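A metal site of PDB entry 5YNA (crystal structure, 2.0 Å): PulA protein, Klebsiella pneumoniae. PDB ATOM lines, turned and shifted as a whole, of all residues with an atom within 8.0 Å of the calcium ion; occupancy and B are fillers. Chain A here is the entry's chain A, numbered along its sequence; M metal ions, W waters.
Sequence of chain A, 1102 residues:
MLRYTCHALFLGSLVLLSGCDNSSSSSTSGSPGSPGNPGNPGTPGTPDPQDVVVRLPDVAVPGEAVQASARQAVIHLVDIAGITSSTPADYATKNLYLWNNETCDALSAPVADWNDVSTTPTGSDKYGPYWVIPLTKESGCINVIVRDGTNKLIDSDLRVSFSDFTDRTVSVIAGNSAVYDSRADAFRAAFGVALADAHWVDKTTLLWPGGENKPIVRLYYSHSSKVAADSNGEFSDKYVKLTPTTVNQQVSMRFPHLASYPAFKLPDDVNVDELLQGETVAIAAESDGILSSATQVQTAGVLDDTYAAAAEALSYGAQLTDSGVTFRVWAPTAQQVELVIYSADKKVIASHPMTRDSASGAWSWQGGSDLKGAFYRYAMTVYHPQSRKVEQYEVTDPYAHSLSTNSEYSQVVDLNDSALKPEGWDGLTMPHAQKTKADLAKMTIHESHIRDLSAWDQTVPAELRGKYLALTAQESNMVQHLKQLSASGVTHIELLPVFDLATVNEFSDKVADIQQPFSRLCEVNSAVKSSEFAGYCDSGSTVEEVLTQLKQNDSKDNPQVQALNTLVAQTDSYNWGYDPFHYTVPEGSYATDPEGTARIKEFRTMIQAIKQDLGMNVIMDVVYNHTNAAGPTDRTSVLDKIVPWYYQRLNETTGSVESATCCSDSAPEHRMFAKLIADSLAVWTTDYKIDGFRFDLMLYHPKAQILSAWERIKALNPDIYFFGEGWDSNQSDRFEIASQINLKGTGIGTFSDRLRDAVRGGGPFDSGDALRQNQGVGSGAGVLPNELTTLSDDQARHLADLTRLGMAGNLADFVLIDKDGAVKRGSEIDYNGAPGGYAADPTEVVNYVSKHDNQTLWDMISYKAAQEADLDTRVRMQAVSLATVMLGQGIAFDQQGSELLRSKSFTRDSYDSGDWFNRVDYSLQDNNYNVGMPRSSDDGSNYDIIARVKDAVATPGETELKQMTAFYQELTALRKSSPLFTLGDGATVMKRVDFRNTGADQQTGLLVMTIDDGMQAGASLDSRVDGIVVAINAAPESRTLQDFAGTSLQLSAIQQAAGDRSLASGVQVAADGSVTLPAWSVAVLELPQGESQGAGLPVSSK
OG of Ser 407 is in hydrogen-bond range of OD2 of Asp 500. O of Asp 500 sits at hydrogen-bond distance from N of Phe 581, at 2.8 Å. A ring nitrogen (ND1) of His 582 sits at hydrogen-bond distance from the side-chain carboxylate (OD2) of Asp 500, 2.9 Å away. The backbone NH of Asp 500 lies within hydrogen-bond range of the backbone carbonyl oxygen of Val 585, at 2.8 Å. The backbone NH of Gly 588 sits close to the side-chain carboxylate of Glu 506 (3.0 Å). N of Glu 506 lies within hydrogen-bond range of OD1 of Asn 406, at 2.9 Å. OE1 of Glu 506 lies within salt-bridge range of NH2 of Arg 599 (3.5 Å). The side-chain carboxylate (OE1) of Glu 587 sits at hydrogen-bond distance from the side-chain hydroxyl (OG) of Ser 589, at 2.7 Å.
The side-chain carboxylate (OD1) of Asp 500 binds the calcium ion, at 2.2 Å. The calcium ion is bound by OE2 of Glu 506 (2.2 Å). Water W2 is bound to the calcium ion (2.3 Å). The calcium ion is bound by the side-chain carboxylate (OE2) of Glu 587. O of Leu 501 binds the calcium ion. Water W1 is bound to the calcium ion.
Merely in contact with the calcium ion: Ser 407. Of the 26 residues printed, 5 come within 4 Å of the calcium ion. The nearest printed residue that does not touch the calcium ion is Gly 588 (4.3 Å).
Water W2 lies within hydrogen-bond range of O of Val 504 and OE1 of Glu 587.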
ATOM      1  N   LEU A 403     -16.493 -20.819  22.252  1.00  0.00           N
ATOM      2  CA  LEU A 403     -15.441 -19.904  22.674  1.00  0.00           C
ATOM      3  C   LEU A 403     -14.614 -19.437  21.482  1.00  0.00           C
ATOM      4  O   LEU A 403     -14.577 -20.078  20.437  1.00  0.00           O
ATOM      5  CB  LEU A 403     -14.504 -20.572  23.696  1.00  0.00           C
ATOM      6  CG  LEU A 403     -15.122 -20.783  25.087  1.00  0.00           C
ATOM      7  CD1 LEU A 403     -14.328 -21.849  25.837  1.00  0.00           C
ATOM      8  CD2 LEU A 403     -15.129 -19.471  25.884  1.00  0.00           C
ATOM      9  N   SER A 404     -13.958 -18.288  21.674  1.00  0.00           N
ATOM     10  CA  SER A 404     -12.896 -17.854  20.785  1.00  0.00           C
ATOM     11  C   SER A 404     -11.604 -18.602  21.132  1.00  0.00           C
ATOM     12  O   SER A 404     -11.543 -19.389  22.086  1.00  0.00           O
ATOM     13  CB  SER A 404     -12.699 -16.339  20.905  1.00  0.00           C
ATOM     14  OG  SER A 404     -12.049 -15.986  22.112  1.00  0.00           O
ATOM     15  N   THR A 405     -10.555 -18.342  20.365  1.00  0.00           N
ATOM     16  CA  THR A 405      -9.278 -19.000  20.605  1.00  0.00           C
ATOM     17  C   THR A 405      -8.748 -18.684  21.998  1.00  0.00           C
ATOM     18  O   THR A 405      -8.718 -17.525  22.424  1.00  0.00           O
ATOM     19  CB  THR A 405      -8.249 -18.589  19.545  1.00  0.00           C
ATOM     20  OG1 THR A 405      -8.720 -18.989  18.252  1.00  0.00           O
ATOM     21  CG2 THR A 405      -6.906 -19.279  19.801  1.00  0.00           C
ATOM     22  N   ASN A 406      -8.356 -19.740  22.726  1.00  0.00           N
ATOM     23  CA  ASN A 406      -7.821 -19.655  24.085  1.00  0.00           C
ATOM     24  C   ASN A 406      -8.855 -19.149  25.099  1.00  0.00           C
ATOM     25  O   ASN A 406      -8.481 -18.679  26.185  1.00  0.00           O
ATOM     26  CB  ASN A 406      -6.559 -18.781  24.138  1.00  0.00           C
ATOM     27  CG  ASN A 406      -5.487 -19.370  25.034  1.00  0.00           C
ATOM     28  OD1 ASN A 406      -5.386 -20.588  25.158  1.00  0.00           O
ATOM     29  ND2 ASN A 406      -4.711 -18.523  25.681  1.00  0.00           N
ATOM     30  N   SER A 407     -10.138 -19.247  24.765  1.00  0.00           N
ATOM     31  CA  SER A 407     -11.232 -19.020  25.696  1.00  0.00           C
ATOM     32  C   SER A 407     -11.316 -17.563  26.156  1.00  0.00           C
ATOM     33  O   SER A 407     -11.802 -17.281  27.253  1.00  0.00           O
ATOM     34  CB  SER A 407     -11.130 -19.976  26.918  1.00  0.00           C
ATOM     35  OG  SER A 407     -10.730 -21.293  26.542  1.00  0.00           O
ATOM     36  N   PHE A 499     -13.249 -31.276  27.770  1.00  0.00           N
ATOM     37  CA  PHE A 499     -13.796 -29.936  28.014  1.00  0.00           C
ATOM     38  C   PHE A 499     -12.663 -28.926  27.914  1.00  0.00           C
ATOM     39  O   PHE A 499     -11.490 -29.281  27.773  1.00  0.00           O
ATOM     40  CB  PHE A 499     -14.442 -29.859  29.401  1.00  0.00           C
ATOM     41  CG  PHE A 499     -13.515 -30.317  30.500  1.00  0.00           C
ATOM     42  CD1 PHE A 499     -12.607 -29.422  31.062  1.00  0.00           C
ATOM     43  CD2 PHE A 499     -13.515 -31.641  30.927  1.00  0.00           C
ATOM     44  CE1 PHE A 499     -11.721 -29.853  32.040  1.00  0.00           C
ATOM     45  CE2 PHE A 499     -12.635 -32.084  31.910  1.00  0.00           C
ATOM     46  CZ  PHE A 499     -11.744 -31.191  32.484  1.00  0.00           C
ATOM     47  N   ASP A 500     -12.998 -27.639  28.012  1.00  0.00           N
ATOM     48  CA  ASP A 500     -12.007 -26.585  27.825  1.00  0.00           C
ATOM     49  C   ASP A 500     -11.040 -26.535  29.003  1.00  0.00           C
ATOM     50  O   ASP A 500     -11.383 -26.013  30.066  1.00  0.00           O
ATOM     51  CB  ASP A 500     -12.691 -25.218  27.661  1.00  0.00           C
ATOM     52  CG  ASP A 500     -11.678 -24.112  27.479  1.00  0.00           C
ATOM     53  OD1 ASP A 500     -10.658 -24.391  26.814  1.00  0.00           O
ATOM     54  OD2 ASP A 500     -11.893 -22.984  27.972  1.00  0.00           O
ATOM     55  N   LEU A 501      -9.818 -27.025  28.801  1.00  0.00           N
ATOM     56  CA  LEU A 501      -8.770 -26.932  29.807  1.00  0.00           C
ATOM     57  C   LEU A 501      -8.010 -25.606  29.676  1.00  0.00           C
ATOM     58  O   LEU A 501      -8.041 -24.945  28.637  1.00  0.00           O
ATOM     59  CB  LEU A 501      -7.792 -28.109  29.710  1.00  0.00           C
ATOM     60  CG  LEU A 501      -7.116 -28.364  28.364  1.00  0.00           C
ATOM     61  CD1 LEU A 501      -5.580 -28.212  28.441  1.00  0.00           C
ATOM     62  CD2 LEU A 501      -7.471 -29.735  27.879  1.00  0.00           C
ATOM     63  N   ALA A 502      -7.328 -25.228  30.760  1.00  0.00           N
ATOM     64  CA  ALA A 502      -6.621 -23.950  30.806  1.00  0.00           C
ATOM     65  C   ALA A 502      -5.147 -24.033  30.392  1.00  0.00           C
ATOM     66  O   ALA A 502      -4.587 -23.012  29.998  1.00  0.00           O
ATOM     67  CB  ALA A 502      -6.677 -23.355  32.212  1.00  0.00           C
ATOM     68  N   THR A 503      -4.519 -25.215  30.495  1.00  0.00           N
ATOM     69  CA  THR A 503      -3.061 -25.325  30.623  1.00  0.00           C
ATOM     70  C   THR A 503      -2.363 -25.679  29.307  1.00  0.00           C
ATOM     71  O   THR A 503      -1.206 -26.118  29.319  1.00  0.00           O
ATOM     72  CB  THR A 503      -2.695 -26.347  31.699  1.00  0.00           C
ATOM     73  OG1 THR A 503      -3.488 -27.534  31.534  1.00  0.00           O
ATOM     74  CG2 THR A 503      -2.929 -25.785  33.111  1.00  0.00           C
ATOM     75  N   VAL A 504      -3.033 -25.501  28.171  1.00  0.00           N
ATOM     76  CA  VAL A 504      -2.409 -25.501  26.854  1.00  0.00           C
ATOM     77  C   VAL A 504      -2.791 -24.192  26.185  1.00  0.00           C
ATOM     78  O   VAL A 504      -3.959 -23.795  26.221  1.00  0.00           O
ATOM     79  CB  VAL A 504      -2.873 -26.701  25.990  1.00  0.00           C
ATOM     80  CG1 VAL A 504      -2.374 -26.564  24.541  1.00  0.00           C
ATOM     81  CG2 VAL A 504      -2.382 -28.015  26.619  1.00  0.00           C
ATOM     82  N   ASN A 505      -1.819 -23.521  25.575  1.00  0.00           N
ATOM     83  CA  ASN A 505      -2.121 -22.292  24.867  1.00  0.00           C
ATOM     84  C   ASN A 505      -2.711 -22.606  23.493  1.00  0.00           C
ATOM     85  O   ASN A 505      -2.080 -23.285  22.680  1.00  0.00           O
ATOM     86  CB  ASN A 505      -0.867 -21.418  24.754  1.00  0.00           C
ATOM     87  CG  ASN A 505      -1.190 -20.003  24.342  1.00  0.00           C
ATOM     88  OD1 ASN A 505      -2.065 -19.803  23.509  1.00  0.00           O
ATOM     89  ND2 ASN A 505      -0.478 -19.022  24.925  1.00  0.00           N
ATOM     90  N   GLU A 506      -3.929 -22.111  23.236  1.00  0.00           N
ATOM     91  CA  GLU A 506      -4.606 -22.437  21.998  1.00  0.00           C
ATOM     92  C   GLU A 506      -4.189 -21.548  20.831  1.00  0.00           C
ATOM     93  O   GLU A 506      -4.668 -21.769  19.714  1.00  0.00           O
ATOM     94  CB  GLU A 506      -6.126 -22.348  22.211  1.00  0.00           C
ATOM     95  CG  GLU A 506      -6.613 -23.336  23.263  1.00  0.00           C
ATOM     96  CD  GLU A 506      -8.132 -23.407  23.414  1.00  0.00           C
ATOM     97  OE1 GLU A 506      -8.862 -22.676  22.707  1.00  0.00           O
ATOM     98  OE2 GLU A 506      -8.602 -24.209  24.231  1.00  0.00           O
ATOM     99  N   ASP A 579      -7.692 -29.228  34.438  1.00  0.00           N
ATOM    100  CA  ASP A 579      -7.501 -27.805  34.741  1.00  0.00           C
ATOM    101  C   ASP A 579      -8.631 -27.014  34.092  1.00  0.00           C
ATOM    102  O   ASP A 579      -8.453 -26.398  33.043  1.00  0.00           O
ATOM    103  CB  ASP A 579      -6.147 -27.298  34.217  1.00  0.00           C
ATOM    104  CG  ASP A 579      -4.976 -28.113  34.729  1.00  0.00           C
ATOM    105  OD1 ASP A 579      -4.721 -28.082  35.947  1.00  0.00           O
ATOM    106  OD2 ASP A 579      -4.267 -28.762  33.908  1.00  0.00           O
ATOM    107  N   PRO A 580      -9.825 -27.039  34.684  1.00  0.00           N
ATOM    108  CA  PRO A 580     -11.032 -26.579  33.956  1.00  0.00           C
ATOM    109  C   PRO A 580     -11.038 -25.066  33.778  1.00  0.00           C
ATOM    110  O   PRO A 580     -10.863 -24.317  34.724  1.00  0.00           O
ATOM    111  CB  PRO A 580     -12.181 -27.034  34.858  1.00  0.00           C
ATOM    112  CG  PRO A 580     -11.582 -28.136  35.726  1.00  0.00           C
ATOM    113  CD  PRO A 580     -10.174 -27.689  35.956  1.00  0.00           C
ATOM    114  N   PHE A 581     -11.250 -24.648  32.530  1.00  0.00           N
ATOM    115  CA  PHE A 581     -11.449 -23.239  32.202  1.00  0.00           C
ATOM    116  C   PHE A 581     -12.935 -22.960  31.982  1.00  0.00           C
ATOM    117  O   PHE A 581     -13.517 -22.132  32.685  1.00  0.00           O
ATOM    118  CB  PHE A 581     -10.586 -22.887  30.970  1.00  0.00           C
ATOM    119  CG  PHE A 581     -10.241 -21.402  30.827  1.00  0.00           C
ATOM    120  CD1 PHE A 581     -10.898 -20.433  31.573  1.00  0.00           C
ATOM    121  CD2 PHE A 581      -9.275 -21.010  29.900  1.00  0.00           C
ATOM    122  CE1 PHE A 581     -10.600 -19.063  31.411  1.00  0.00           C
ATOM    123  CE2 PHE A 581      -8.967 -19.639  29.718  1.00  0.00           C
ATOM    124  CZ  PHE A 581      -9.629 -18.671  30.492  1.00  0.00           C
ATOM    125  N   HIS A 582     -13.578 -23.698  31.059  1.00  0.00           N
ATOM    126  CA  HIS A 582     -15.028 -23.707  30.886  1.00  0.00           C
ATOM    127  C   HIS A 582     -15.535 -25.141  30.832  1.00  0.00           C
ATOM    128  O   HIS A 582     -15.024 -25.957  30.067  1.00  0.00           O
ATOM    129  CB  HIS A 582     -15.431 -22.980  29.602  1.00  0.00           C
ATOM    130  CG  HIS A 582     -15.010 -21.546  29.605  1.00  0.00           C
ATOM    131  ND1 HIS A 582     -13.728 -21.150  29.289  1.00  0.00           N
ATOM    132  CD2 HIS A 582     -15.679 -20.424  29.967  1.00  0.00           C
ATOM    133  CE1 HIS A 582     -13.637 -19.840  29.415  1.00  0.00           C
ATOM    134  NE2 HIS A 582     -14.804 -19.375  29.825  1.00  0.00           N
ATOM    135  N   VAL A 585     -17.687 -26.425  27.080  1.00  0.00           N
ATOM    136  CA  VAL A 585     -17.186 -26.189  25.721  1.00  0.00           C
ATOM    137  C   VAL A 585     -16.085 -27.207  25.463  1.00  0.00           C
ATOM    138  O   VAL A 585     -15.286 -27.468  26.367  1.00  0.00           O
ATOM    139  CB  VAL A 585     -16.652 -24.760  25.571  1.00  0.00           C
ATOM    140  CG1 VAL A 585     -16.381 -24.440  24.099  1.00  0.00           C
ATOM    141  CG2 VAL A 585     -17.628 -23.748  26.123  1.00  0.00           C
ATOM    142  N   PRO A 586     -15.984 -27.809  24.271  1.00  0.00           N
ATOM    143  CA  PRO A 586     -14.802 -28.645  24.003  1.00  0.00           C
ATOM    144  C   PRO A 586     -13.525 -27.841  24.099  1.00  0.00           C
ATOM    145  O   PRO A 586     -13.507 -26.627  23.916  1.00  0.00           O
ATOM    146  CB  PRO A 586     -15.040 -29.156  22.565  1.00  0.00           C
ATOM    147  CG  PRO A 586     -16.541 -29.142  22.413  1.00  0.00           C
ATOM    148  CD  PRO A 586     -16.977 -27.893  23.189  1.00  0.00           C
ATOM    149  N   GLU A 587     -12.445 -28.534  24.420  1.00  0.00           N
ATOM    150  CA  GLU A 587     -11.110 -27.963  24.347  1.00  0.00           C
ATOM    151  C   GLU A 587     -10.788 -27.516  22.915  1.00  0.00           C
ATOM    152  O   GLU A 587     -11.095 -28.221  21.948  1.00  0.00           O
ATOM    153  CB  GLU A 587     -10.092 -29.008  24.827  1.00  0.00           C
ATOM    154  CG  GLU A 587      -8.640 -28.722  24.485  1.00  0.00           C
ATOM    155  CD  GLU A 587      -8.124 -27.412  25.045  1.00  0.00           C
ATOM    156  OE1 GLU A 587      -7.060 -26.982  24.587  1.00  0.00           O
ATOM    157  OE2 GLU A 587      -8.769 -26.806  25.947  1.00  0.00           O
ATOM    158  N   GLY A 588     -10.127 -26.354  22.807  1.00  0.00           N
ATOM    159  CA  GLY A 588      -9.828 -25.810  21.481  1.00  0.00           C
ATOM    160  C   GLY A 588      -8.564 -26.341  20.833  1.00  0.00           C
ATOM    161  O   GLY A 588      -8.516 -26.465  19.605  1.00  0.00           O
ATOM    162  N   SER A 589      -7.527 -26.631  21.632  1.00  0.00           N
ATOM    163  CA  SER A 589      -6.267 -27.072  21.030  1.00  0.00           C
ATOM    164  C   SER A 589      -6.401 -28.413  20.323  1.00  0.00           C
ATOM    165  O   SER A 589      -5.561 -28.733  19.469  1.00  0.00           O
ATOM    166  CB  SER A 589      -5.165 -27.145  22.096  1.00  0.00           C
ATOM    167  OG  SER A 589      -5.369 -28.247  22.969  1.00  0.00           O
ATOM    168  N   TYR A 590      -7.434 -29.190  20.640  1.00  0.00           N
ATOM    169  CA  TYR A 590      -7.697 -30.457  19.957  1.00  0.00           C
ATOM    170  C   TYR A 590      -8.478 -30.281  18.666  1.00  0.00           C
ATOM    171  O   TYR A 590      -8.728 -31.274  17.965  1.00  0.00           O
ATOM    172  CB  TYR A 590      -8.445 -31.396  20.896  1.00  0.00           C
ATOM    173  CG  TYR A 590      -7.677 -31.744  22.137  1.00  0.00           C
ATOM    174  CD1 TYR A 590      -6.286 -31.851  22.103  1.00  0.00           C
ATOM    175  CD2 TYR A 590      -8.329 -32.008  23.334  1.00  0.00           C
ATOM    176  CE1 TYR A 590      -5.573 -32.195  23.235  1.00  0.00           C
ATOM    177  CE2 TYR A 590      -7.623 -32.364  24.471  1.00  0.00           C
ATOM    178  CZ  TYR A 590      -6.237 -32.451  24.416  1.00  0.00           C
ATOM    179  OH  TYR A 590      -5.542 -32.787  25.559  1.00  0.00           O
ATOM    180  N   PRO A 594      -9.305 -23.471  16.482  1.00  0.00           N
ATOM    181  CA  PRO A 594      -9.844 -23.128  17.809  1.00  0.00           C
ATOM    182  C   PRO A 594     -10.681 -21.842  17.846  1.00  0.00           C
ATOM    183  O   PRO A 594     -11.168 -21.470  18.925  1.00  0.00           O
ATOM    184  CB  PRO A 594      -8.579 -22.976  18.644  1.00  0.00           C
ATOM    185  CG  PRO A 594      -7.558 -22.466  17.643  1.00  0.00           C
ATOM    186  CD  PRO A 594      -7.871 -23.159  16.360  1.00  0.00           C
ATOM    187  N   ARG A 599     -14.777 -26.186  16.582  1.00  0.00           N
ATOM    188  CA  ARG A 599     -14.457 -27.323  17.454  1.00  0.00           C
ATOM    189  C   ARG A 599     -15.693 -28.146  17.772  1.00  0.00           C
ATOM    190  O   ARG A 599     -15.591 -29.365  17.981  1.00  0.00           O
ATOM    191  CB  ARG A 599     -13.808 -26.829  18.736  1.00  0.00           C
ATOM    192  CG  ARG A 599     -14.767 -26.081  19.640  1.00  0.00           C
ATOM    193  CD  ARG A 599     -14.082 -25.593  20.885  1.00  0.00           C
ATOM    194  NE  ARG A 599     -13.283 -24.412  20.628  1.00  0.00           N
ATOM    195  CZ  ARG A 599     -12.718 -23.695  21.594  1.00  0.00           C
ATOM    196  NH1 ARG A 599     -12.854 -24.076  22.865  1.00  0.00           N
ATOM    197  NH2 ARG A 599     -12.017 -22.606  21.304  1.00  0.00           N
ATOM    198  N   ARG A 635      -6.296 -14.876  34.999  1.00  0.00           N
ATOM    199  CA  ARG A 635      -6.931 -15.045  33.693  1.00  0.00           C
ATOM    200  C   ARG A 635      -8.022 -16.120  33.719  1.00  0.00           C
ATOM    201  O   ARG A 635      -9.071 -15.953  33.087  1.00  0.00           O
ATOM    202  CB  ARG A 635      -5.839 -15.392  32.650  1.00  0.00           C
ATOM    203  CG  ARG A 635      -6.316 -16.014  31.342  1.00  0.00           C
ATOM    204  CD  ARG A 635      -5.142 -16.423  30.454  1.00  0.00           C
ATOM    205  NE  ARG A 635      -4.575 -17.716  30.831  1.00  0.00           N
ATOM    206  CZ  ARG A 635      -4.826 -18.861  30.204  1.00  0.00           C
ATOM    207  NH1 ARG A 635      -5.622 -18.881  29.148  1.00  0.00           N
ATOM    208  NH2 ARG A 635      -4.278 -19.995  30.618  1.00  0.00           N
HETATM  209 CA    CA M   1      -8.532 -24.584  26.424  1.00  0.00          CA
HETATM  210  O   HOH W   1      -8.083 -22.302  26.709  1.00  0.00           O
HETATM  211  O   HOH W   2      -6.302 -24.959  26.455  1.00  0.00           O
